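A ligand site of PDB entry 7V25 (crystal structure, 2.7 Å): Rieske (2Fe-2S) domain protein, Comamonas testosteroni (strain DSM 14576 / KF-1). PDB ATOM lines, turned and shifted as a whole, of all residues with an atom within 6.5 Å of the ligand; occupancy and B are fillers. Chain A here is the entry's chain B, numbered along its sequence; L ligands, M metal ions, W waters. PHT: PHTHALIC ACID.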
ATOM      1  N   GLY A 175      21.672   6.335   6.689  1.00  0.00           N
ATOM      2  CA  GLY A 175      22.093   5.779   5.410  1.00  0.00           C
ATOM      3  C   GLY A 175      22.483   4.303   5.491  1.00  0.00           C
ATOM      4  O   GLY A 175      22.436   3.599   4.478  1.00  0.00           O
ATOM      5  N   ALA A 176      22.889   3.855   6.675  1.00  0.00           N
ATOM      6  CA  ALA A 176      23.327   2.474   6.835  1.00  0.00           C
ATOM      7  C   ALA A 176      22.133   1.554   7.025  1.00  0.00           C
ATOM      8  O   ALA A 176      22.265   0.339   6.846  1.00  0.00           O
ATOM      9  CB  ALA A 176      24.313   2.345   7.982  1.00  0.00           C
ATOM     10  N   ILE A 177      20.966   2.109   7.368  1.00  0.00           N
ATOM     11  CA  ILE A 177      19.767   1.316   7.583  1.00  0.00           C
ATOM     12  C   ILE A 177      18.701   1.726   6.557  1.00  0.00           C
ATOM     13  O   ILE A 177      17.664   2.281   6.917  1.00  0.00           O
ATOM     14  CB  ILE A 177      19.276   1.408   9.058  1.00  0.00           C
ATOM     15  CG1 ILE A 177      18.944   2.839   9.506  1.00  0.00           C
ATOM     16  CG2 ILE A 177      20.285   0.766  10.004  1.00  0.00           C
ATOM     17  CD1 ILE A 177      18.378   2.919  10.897  1.00  0.00           C
ATOM     18  N   ASP A 178      18.968   1.430   5.282  1.00  0.00           N
ATOM     19  CA  ASP A 178      18.131   1.992   4.222  1.00  0.00           C
ATOM     20  C   ASP A 178      18.225   1.127   2.968  1.00  0.00           C
ATOM     21  O   ASP A 178      18.504   1.656   1.888  1.00  0.00           O
ATOM     22  CB  ASP A 178      18.591   3.425   3.927  1.00  0.00           C
ATOM     23  CG  ASP A 178      17.655   4.250   3.060  1.00  0.00           C
ATOM     24  OD1 ASP A 178      16.588   3.731   2.645  1.00  0.00           O
ATOM     25  OD2 ASP A 178      18.002   5.417   2.814  1.00  0.00           O
ATOM     26  N   SER A 179      17.946  -0.174   3.109  1.00  0.00           N
ATOM     27  CA  SER A 179      18.193  -1.130   2.032  1.00  0.00           C
ATOM     28  C   SER A 179      17.704  -0.608   0.680  1.00  0.00           C
ATOM     29  O   SER A 179      18.247  -0.973  -0.366  1.00  0.00           O
ATOM     30  CB  SER A 179      17.613  -2.493   2.342  1.00  0.00           C
ATOM     31  OG  SER A 179      18.453  -3.516   1.833  1.00  0.00           O
ATOM     32  N   ALA A 180      16.693   0.262   0.723  1.00  0.00           N
ATOM     33  CA  ALA A 180      16.068   0.853  -0.441  1.00  0.00           C
ATOM     34  C   ALA A 180      17.100   1.563  -1.328  1.00  0.00           C
ATOM     35  O   ALA A 180      17.104   1.401  -2.546  1.00  0.00           O
ATOM     36  CB  ALA A 180      14.998   1.821   0.022  1.00  0.00           C
ATOM     37  N   HIS A 181      17.962   2.351  -0.695  1.00  0.00           N
ATOM     38  CA  HIS A 181      18.828   3.303  -1.385  1.00  0.00           C
ATOM     39  C   HIS A 181      19.797   2.551  -2.300  1.00  0.00           C
ATOM     40  O   HIS A 181      20.217   3.063  -3.332  1.00  0.00           O
ATOM     41  CB  HIS A 181      19.515   4.240  -0.386  1.00  0.00           C
ATOM     42  CG  HIS A 181      20.836   3.781   0.136  1.00  0.00           C
ATOM     43  ND1 HIS A 181      20.950   2.967   1.250  1.00  0.00           N
ATOM     44  CD2 HIS A 181      22.095   4.016  -0.287  1.00  0.00           C
ATOM     45  CE1 HIS A 181      22.223   2.723   1.487  1.00  0.00           C
ATOM     46  NE2 HIS A 181      22.942   3.350   0.558  1.00  0.00           N
ATOM     47  N   SER A 182      20.141   1.335  -1.905  1.00  0.00           N
ATOM     48  CA  SER A 182      21.167   0.628  -2.638  1.00  0.00           C
ATOM     49  C   SER A 182      20.685   0.274  -4.040  1.00  0.00           C
ATOM     50  O   SER A 182      21.478   0.189  -4.982  1.00  0.00           O
ATOM     51  CB  SER A 182      21.642  -0.549  -1.847  1.00  0.00           C
ATOM     52  OG  SER A 182      22.452  -0.107  -0.763  1.00  0.00           O
ATOM     53  N   HIS A 186      23.241   2.920  -5.386  1.00  0.00           N
ATOM     54  CA  HIS A 186      24.339   2.005  -5.661  1.00  0.00           C
ATOM     55  C   HIS A 186      23.943   1.017  -6.777  1.00  0.00           C
ATOM     56  O   HIS A 186      24.432  -0.111  -6.814  1.00  0.00           O
ATOM     57  CB  HIS A 186      24.900   1.332  -4.393  1.00  0.00           C
ATOM     58  CG  HIS A 186      25.133   2.207  -3.192  1.00  0.00           C
ATOM     59  ND1 HIS A 186      25.796   3.430  -3.257  1.00  0.00           N
ATOM     60  CD2 HIS A 186      24.815   2.018  -1.893  1.00  0.00           C
ATOM     61  CE1 HIS A 186      25.839   3.964  -2.048  1.00  0.00           C
ATOM     62  NE2 HIS A 186      25.240   3.111  -1.189  1.00  0.00           N
ATOM     63  N   MET A 190      26.495  -2.240  -6.871  1.00  0.00           N
ATOM     64  CA  MET A 190      25.947  -3.514  -6.438  1.00  0.00           C
ATOM     65  C   MET A 190      24.924  -3.938  -7.482  1.00  0.00           C
ATOM     66  O   MET A 190      23.760  -3.553  -7.402  1.00  0.00           O
ATOM     67  CB  MET A 190      25.327  -3.397  -5.042  1.00  0.00           C
ATOM     68  CG  MET A 190      26.298  -2.849  -3.993  1.00  0.00           C
ATOM     69  SD  MET A 190      25.463  -2.073  -2.577  1.00  0.00           S
ATOM     70  CE  MET A 190      26.841  -1.231  -1.797  1.00  0.00           C
ATOM     71  N   TRP A 205      30.421  -6.249  -6.199  1.00  0.00           N
ATOM     72  CA  TRP A 205      29.337  -6.862  -5.442  1.00  0.00           C
ATOM     73  C   TRP A 205      28.161  -7.159  -6.375  1.00  0.00           C
ATOM     74  O   TRP A 205      28.102  -6.640  -7.489  1.00  0.00           O
ATOM     75  CB  TRP A 205      28.937  -5.990  -4.244  1.00  0.00           C
ATOM     76  CG  TRP A 205      29.886  -5.974  -3.078  1.00  0.00           C
ATOM     77  CD1 TRP A 205      31.073  -6.640  -2.979  1.00  0.00           C
ATOM     78  CD2 TRP A 205      29.745  -5.234  -1.855  1.00  0.00           C
ATOM     79  NE1 TRP A 205      31.667  -6.372  -1.773  1.00  0.00           N
ATOM     80  CE2 TRP A 205      30.875  -5.512  -1.066  1.00  0.00           C
ATOM     81  CE3 TRP A 205      28.776  -4.354  -1.337  1.00  0.00           C
ATOM     82  CZ2 TRP A 205      31.070  -4.952   0.202  1.00  0.00           C
ATOM     83  CZ3 TRP A 205      28.958  -3.806  -0.083  1.00  0.00           C
ATOM     84  CH2 TRP A 205      30.095  -4.106   0.669  1.00  0.00           C
ATOM     85  N   ARG A 207      23.842  -8.845  -6.661  1.00  0.00           N
ATOM     86  CA  ARG A 207      22.546  -9.089  -6.029  1.00  0.00           C
ATOM     87  C   ARG A 207      21.716 -10.094  -6.833  1.00  0.00           C
ATOM     88  O   ARG A 207      21.599  -9.951  -8.047  1.00  0.00           O
ATOM     89  CB  ARG A 207      21.778  -7.786  -5.837  1.00  0.00           C
ATOM     90  CG  ARG A 207      22.481  -6.772  -4.938  1.00  0.00           C
ATOM     91  CD  ARG A 207      22.703  -7.301  -3.534  1.00  0.00           C
ATOM     92  NE  ARG A 207      23.876  -6.747  -2.882  1.00  0.00           N
ATOM     93  CZ  ARG A 207      23.903  -5.595  -2.219  1.00  0.00           C
ATOM     94  NH1 ARG A 207      25.030  -5.181  -1.654  1.00  0.00           N
ATOM     95  NH2 ARG A 207      22.815  -4.852  -2.129  1.00  0.00           N
ATOM     96  N   TYR A 227      16.098  -5.767  11.439  1.00  0.00           N
ATOM     97  CA  TYR A 227      15.070  -5.690  10.414  1.00  0.00           C
ATOM     98  C   TYR A 227      15.556  -6.425   9.174  1.00  0.00           C
ATOM     99  O   TYR A 227      16.750  -6.669   9.015  1.00  0.00           O
ATOM    100  CB  TYR A 227      14.677  -4.245  10.058  1.00  0.00           C
ATOM    101  CG  TYR A 227      15.470  -3.627   8.936  1.00  0.00           C
ATOM    102  CD1 TYR A 227      16.699  -3.023   9.201  1.00  0.00           C
ATOM    103  CD2 TYR A 227      14.999  -3.611   7.640  1.00  0.00           C
ATOM    104  CE1 TYR A 227      17.437  -2.423   8.194  1.00  0.00           C
ATOM    105  CE2 TYR A 227      15.732  -3.025   6.614  1.00  0.00           C
ATOM    106  CZ  TYR A 227      16.963  -2.430   6.889  1.00  0.00           C
ATOM    107  OH  TYR A 227      17.714  -1.836   5.911  1.00  0.00           O
ATOM    108  N   ARG A 231      13.029  -9.120  -0.796  1.00  0.00           N
ATOM    109  CA  ARG A 231      12.947  -8.861  -2.217  1.00  0.00           C
ATOM    110  C   ARG A 231      12.480 -10.132  -2.948  1.00  0.00           C
ATOM    111  O   ARG A 231      12.857 -11.244  -2.572  1.00  0.00           O
ATOM    112  CB  ARG A 231      14.304  -8.409  -2.768  1.00  0.00           C
ATOM    113  CG  ARG A 231      14.672  -6.969  -2.427  1.00  0.00           C
ATOM    114  CD  ARG A 231      15.658  -6.872  -1.281  1.00  0.00           C
ATOM    115  NE  ARG A 231      16.022  -5.492  -0.966  1.00  0.00           N
ATOM    116  CZ  ARG A 231      16.833  -4.729  -1.696  1.00  0.00           C
ATOM    117  NH1 ARG A 231      17.401  -5.201  -2.791  1.00  0.00           N
ATOM    118  NH2 ARG A 231      17.068  -3.477  -1.316  1.00  0.00           N
ATOM    119  N   ARG A 244      17.288  -9.759   3.346  1.00  0.00           N
ATOM    120  CA  ARG A 244      18.519  -9.087   3.741  1.00  0.00           C
ATOM    121  C   ARG A 244      18.340  -8.456   5.115  1.00  0.00           C
ATOM    122  O   ARG A 244      17.684  -7.424   5.259  1.00  0.00           O
ATOM    123  CB  ARG A 244      18.919  -8.059   2.688  1.00  0.00           C
ATOM    124  CG  ARG A 244      19.308  -8.675   1.352  1.00  0.00           C
ATOM    125  CD  ARG A 244      19.704  -7.629   0.323  1.00  0.00           C
ATOM    126  NE  ARG A 244      21.130  -7.348   0.355  1.00  0.00           N
ATOM    127  CZ  ARG A 244      21.670  -6.234   0.827  1.00  0.00           C
ATOM    128  NH1 ARG A 244      22.996  -6.090   0.806  1.00  0.00           N
ATOM    129  NH2 ARG A 244      20.915  -5.272   1.316  1.00  0.00           N
ATOM    130  N   THR A 246      19.598  -6.441   8.211  1.00  0.00           N
ATOM    131  CA  THR A 246      20.506  -5.530   8.874  1.00  0.00           C
ATOM    132  C   THR A 246      20.162  -5.463  10.371  1.00  0.00           C
ATOM    133  O   THR A 246      18.996  -5.552  10.759  1.00  0.00           O
ATOM    134  CB  THR A 246      20.337  -4.106   8.320  1.00  0.00           C
ATOM    135  OG1 THR A 246      20.693  -4.091   6.937  1.00  0.00           O
ATOM    136  CG2 THR A 246      21.092  -3.053   9.104  1.00  0.00           C
ATOM    137  N   ILE A 256      25.607  -4.519   8.602  1.00  0.00           N
ATOM    138  CA  ILE A 256      25.217  -4.522   7.202  1.00  0.00           C
ATOM    139  C   ILE A 256      25.213  -5.972   6.732  1.00  0.00           C
ATOM    140  O   ILE A 256      26.051  -6.763   7.188  1.00  0.00           O
ATOM    141  CB  ILE A 256      26.221  -3.669   6.373  1.00  0.00           C
ATOM    142  CG1 ILE A 256      26.488  -2.297   6.989  1.00  0.00           C
ATOM    143  CG2 ILE A 256      25.845  -3.541   4.916  1.00  0.00           C
ATOM    144  CD1 ILE A 256      25.283  -1.394   7.072  1.00  0.00           C
ATOM    145  N   PRO A 257      24.313  -6.358   5.798  1.00  0.00           N
ATOM    146  CA  PRO A 257      24.252  -7.747   5.332  1.00  0.00           C
ATOM    147  C   PRO A 257      25.591  -8.148   4.709  1.00  0.00           C
ATOM    148  O   PRO A 257      26.167  -7.409   3.922  1.00  0.00           O
ATOM    149  CB  PRO A 257      23.142  -7.746   4.259  1.00  0.00           C
ATOM    150  CG  PRO A 257      22.350  -6.480   4.527  1.00  0.00           C
ATOM    151  CD  PRO A 257      23.321  -5.494   5.134  1.00  0.00           C
ATOM    152  N   PRO A 258      26.154  -9.326   5.077  1.00  0.00           N
ATOM    153  CA  PRO A 258      27.376  -9.792   4.448  1.00  0.00           C
ATOM    154  C   PRO A 258      27.186 -10.150   2.981  1.00  0.00           C
ATOM    155  O   PRO A 258      26.117  -9.993   2.402  1.00  0.00           O
ATOM    156  CB  PRO A 258      27.762 -11.025   5.297  1.00  0.00           C
ATOM    157  CG  PRO A 258      26.468 -11.503   5.894  1.00  0.00           C
ATOM    158  CD  PRO A 258      25.660 -10.245   6.115  1.00  0.00           C
ATOM    159  N   VAL A 264      30.286  -7.014   6.905  1.00  0.00           N
ATOM    160  CA  VAL A 264      30.437  -5.589   6.653  1.00  0.00           C
ATOM    161  C   VAL A 264      29.768  -4.840   7.789  1.00  0.00           C
ATOM    162  O   VAL A 264      28.630  -5.152   8.138  1.00  0.00           O
ATOM    163  CB  VAL A 264      29.789  -5.214   5.304  1.00  0.00           C
ATOM    164  CG1 VAL A 264      29.849  -3.719   5.051  1.00  0.00           C
ATOM    165  CG2 VAL A 264      30.445  -5.960   4.164  1.00  0.00           C
ATOM    166  N   ASN A 266      29.375  -0.814   9.994  1.00  0.00           N
ATOM    167  CA  ASN A 266      29.570   0.620  10.017  1.00  0.00           C
ATOM    168  C   ASN A 266      29.483   1.037  11.488  1.00  0.00           C
ATOM    169  O   ASN A 266      28.544   0.639  12.161  1.00  0.00           O
ATOM    170  CB  ASN A 266      28.501   1.324   9.159  1.00  0.00           C
ATOM    171  CG  ASN A 266      28.469   2.840   9.282  1.00  0.00           C
ATOM    172  OD1 ASN A 266      29.294   3.431   9.981  1.00  0.00           O
ATOM    173  ND2 ASN A 266      27.531   3.476   8.587  1.00  0.00           N
ATOM    174  N   PHE A 280      34.131   2.209   8.347  1.00  0.00           N
ATOM    175  CA  PHE A 280      33.439   1.248   7.493  1.00  0.00           C
ATOM    176  C   PHE A 280      34.343   0.030   7.282  1.00  0.00           C
ATOM    177  O   PHE A 280      35.412   0.117   6.671  1.00  0.00           O
ATOM    178  CB  PHE A 280      32.975   1.919   6.203  1.00  0.00           C
ATOM    179  CG  PHE A 280      31.975   1.144   5.394  1.00  0.00           C
ATOM    180  CD1 PHE A 280      30.677   0.967   5.833  1.00  0.00           C
ATOM    181  CD2 PHE A 280      32.311   0.633   4.148  1.00  0.00           C
ATOM    182  CE1 PHE A 280      29.746   0.288   5.054  1.00  0.00           C
ATOM    183  CE2 PHE A 280      31.380  -0.046   3.368  1.00  0.00           C
ATOM    184  CZ  PHE A 280      30.087  -0.222   3.816  1.00  0.00           C
ATOM    185  N   PHE A 339      31.420   3.488  -3.756  1.00  0.00           N
ATOM    186  CA  PHE A 339      30.013   3.515  -3.391  1.00  0.00           C
ATOM    187  C   PHE A 339      29.770   4.334  -2.104  1.00  0.00           C
ATOM    188  O   PHE A 339      28.744   5.000  -1.995  1.00  0.00           O
ATOM    189  CB  PHE A 339      29.417   2.109  -3.415  1.00  0.00           C
ATOM    190  CG  PHE A 339      29.587   1.275  -2.158  1.00  0.00           C
ATOM    191  CD1 PHE A 339      29.053   1.697  -0.937  1.00  0.00           C
ATOM    192  CD2 PHE A 339      30.236   0.038  -2.194  1.00  0.00           C
ATOM    193  CE1 PHE A 339      29.202   0.939   0.220  1.00  0.00           C
ATOM    194  CE2 PHE A 339      30.371  -0.718  -1.041  1.00  0.00           C
ATOM    195  CZ  PHE A 339      29.850  -0.281   0.170  1.00  0.00           C
ATOM    196  N   ASP A 343      27.164   7.896  -1.069  1.00  0.00           N
ATOM    197  CA  ASP A 343      26.370   8.210   0.117  1.00  0.00           C
ATOM    198  C   ASP A 343      26.723   9.608   0.645  1.00  0.00           C
ATOM    199  O   ASP A 343      25.853  10.385   1.046  1.00  0.00           O
ATOM    200  CB  ASP A 343      26.513   7.128   1.184  1.00  0.00           C
ATOM    201  CG  ASP A 343      25.831   5.805   0.864  1.00  0.00           C
ATOM    202  OD1 ASP A 343      26.560   4.805   0.720  1.00  0.00           O
ATOM    203  OD2 ASP A 343      24.571   5.749   0.803  1.00  0.00           O
HETATM  204  O8  PHT L   1      25.132  -3.753   0.959  1.00  0.00           O
HETATM  205  O9  PHT L   1      23.331  -2.737   0.204  1.00  0.00           O
HETATM  206  C10 PHT L   1      22.055  -2.054   3.225  1.00  0.00           C
HETATM  207  O11 PHT L   1      21.201  -1.411   3.899  1.00  0.00           O
HETATM  208  O12 PHT L   1      21.829  -3.156   2.696  1.00  0.00           O
HETATM  209  C7  PHT L   1      24.271  -2.851   1.005  1.00  0.00           C
HETATM  210  C1  PHT L   1      23.751  -0.413   3.954  1.00  0.00           C
HETATM  211  C2  PHT L   1      23.442  -1.433   3.046  1.00  0.00           C
HETATM  212  C3  PHT L   1      24.407  -1.790   2.079  1.00  0.00           C
HETATM  213  C4  PHT L   1      25.625  -1.101   2.050  1.00  0.00           C
HETATM  214  C5  PHT L   1      25.902  -0.094   2.955  1.00  0.00           C
HETATM  215  C6  PHT L   1      24.969   0.248   3.905  1.00  0.00           C
HETATM  216 FE    FE M   1      24.939   3.537   0.802  1.00  0.00          FE
HETATM  217  O   HOH W   1      25.732   2.707   2.289  1.00  0.00           O
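The guanidinium group (NH1) of Arg 207 lies within salt-bridge range of an oxygen (O8) of the ligand.
The side-chain hydroxyl of Ser 182 is in hydrogen-bond range of an oxygen (O9) of the ligand, at 2.9 Å.
NH2 of Arg 244 is in salt-bridge range of O12 of the ligand, at 2.7 Å.
The guanidinium group of Arg 231 is in hydrogen-bond range of the backbone carbonyl oxygen of Ser 179 (2.9 Å).
OG of Ser 179 sits at hydrogen-bond distance from NH2 of Arg 244 (3.1 Å).
The backbone carbonyl oxygen (O) of Asp 178 sits at hydrogen-bond distance from a ring nitrogen (ND1) of His 181 (2.8 Å).
N of Ile 256 lies within hydrogen-bond range of O of Val 264 (3.1 Å).
SD of Met 190 sits at hydrogen-bond distance from NH1 of Arg 207 (3.3 Å).
The backbone NH (N) of Ser 179 is in hydrogen-bond range of the side-chain hydroxyl (OH) of Tyr 227 (3.3 Å).
An oxygen (O9) of the ligand lies close to the side-chain sulfur of Met 190 (3.6 Å).
Ala 176 touches the ligand (O to C1, 3.3 Å).
Asp 178 touches the ligand.
OG of Ser 179 touches O12 of the ligand, 3.5 Å away.
Trp 205 touches the ligand.
Ile 256 touches the ligand (CD1 to C6, 3.6 Å).
Pro 257 touches the ligand (CD to O12, 3.7 Å).
Hydrophobic or aromatic side chains that line the ligand: Met 190, Trp 205, Ile 256 and Pro 257.
Along chain A the residues within 4 Å of the ligand span positions 176 to 257.
The nearest printed residue that does not touch the ligand is Tyr 227 (4.05 Å).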
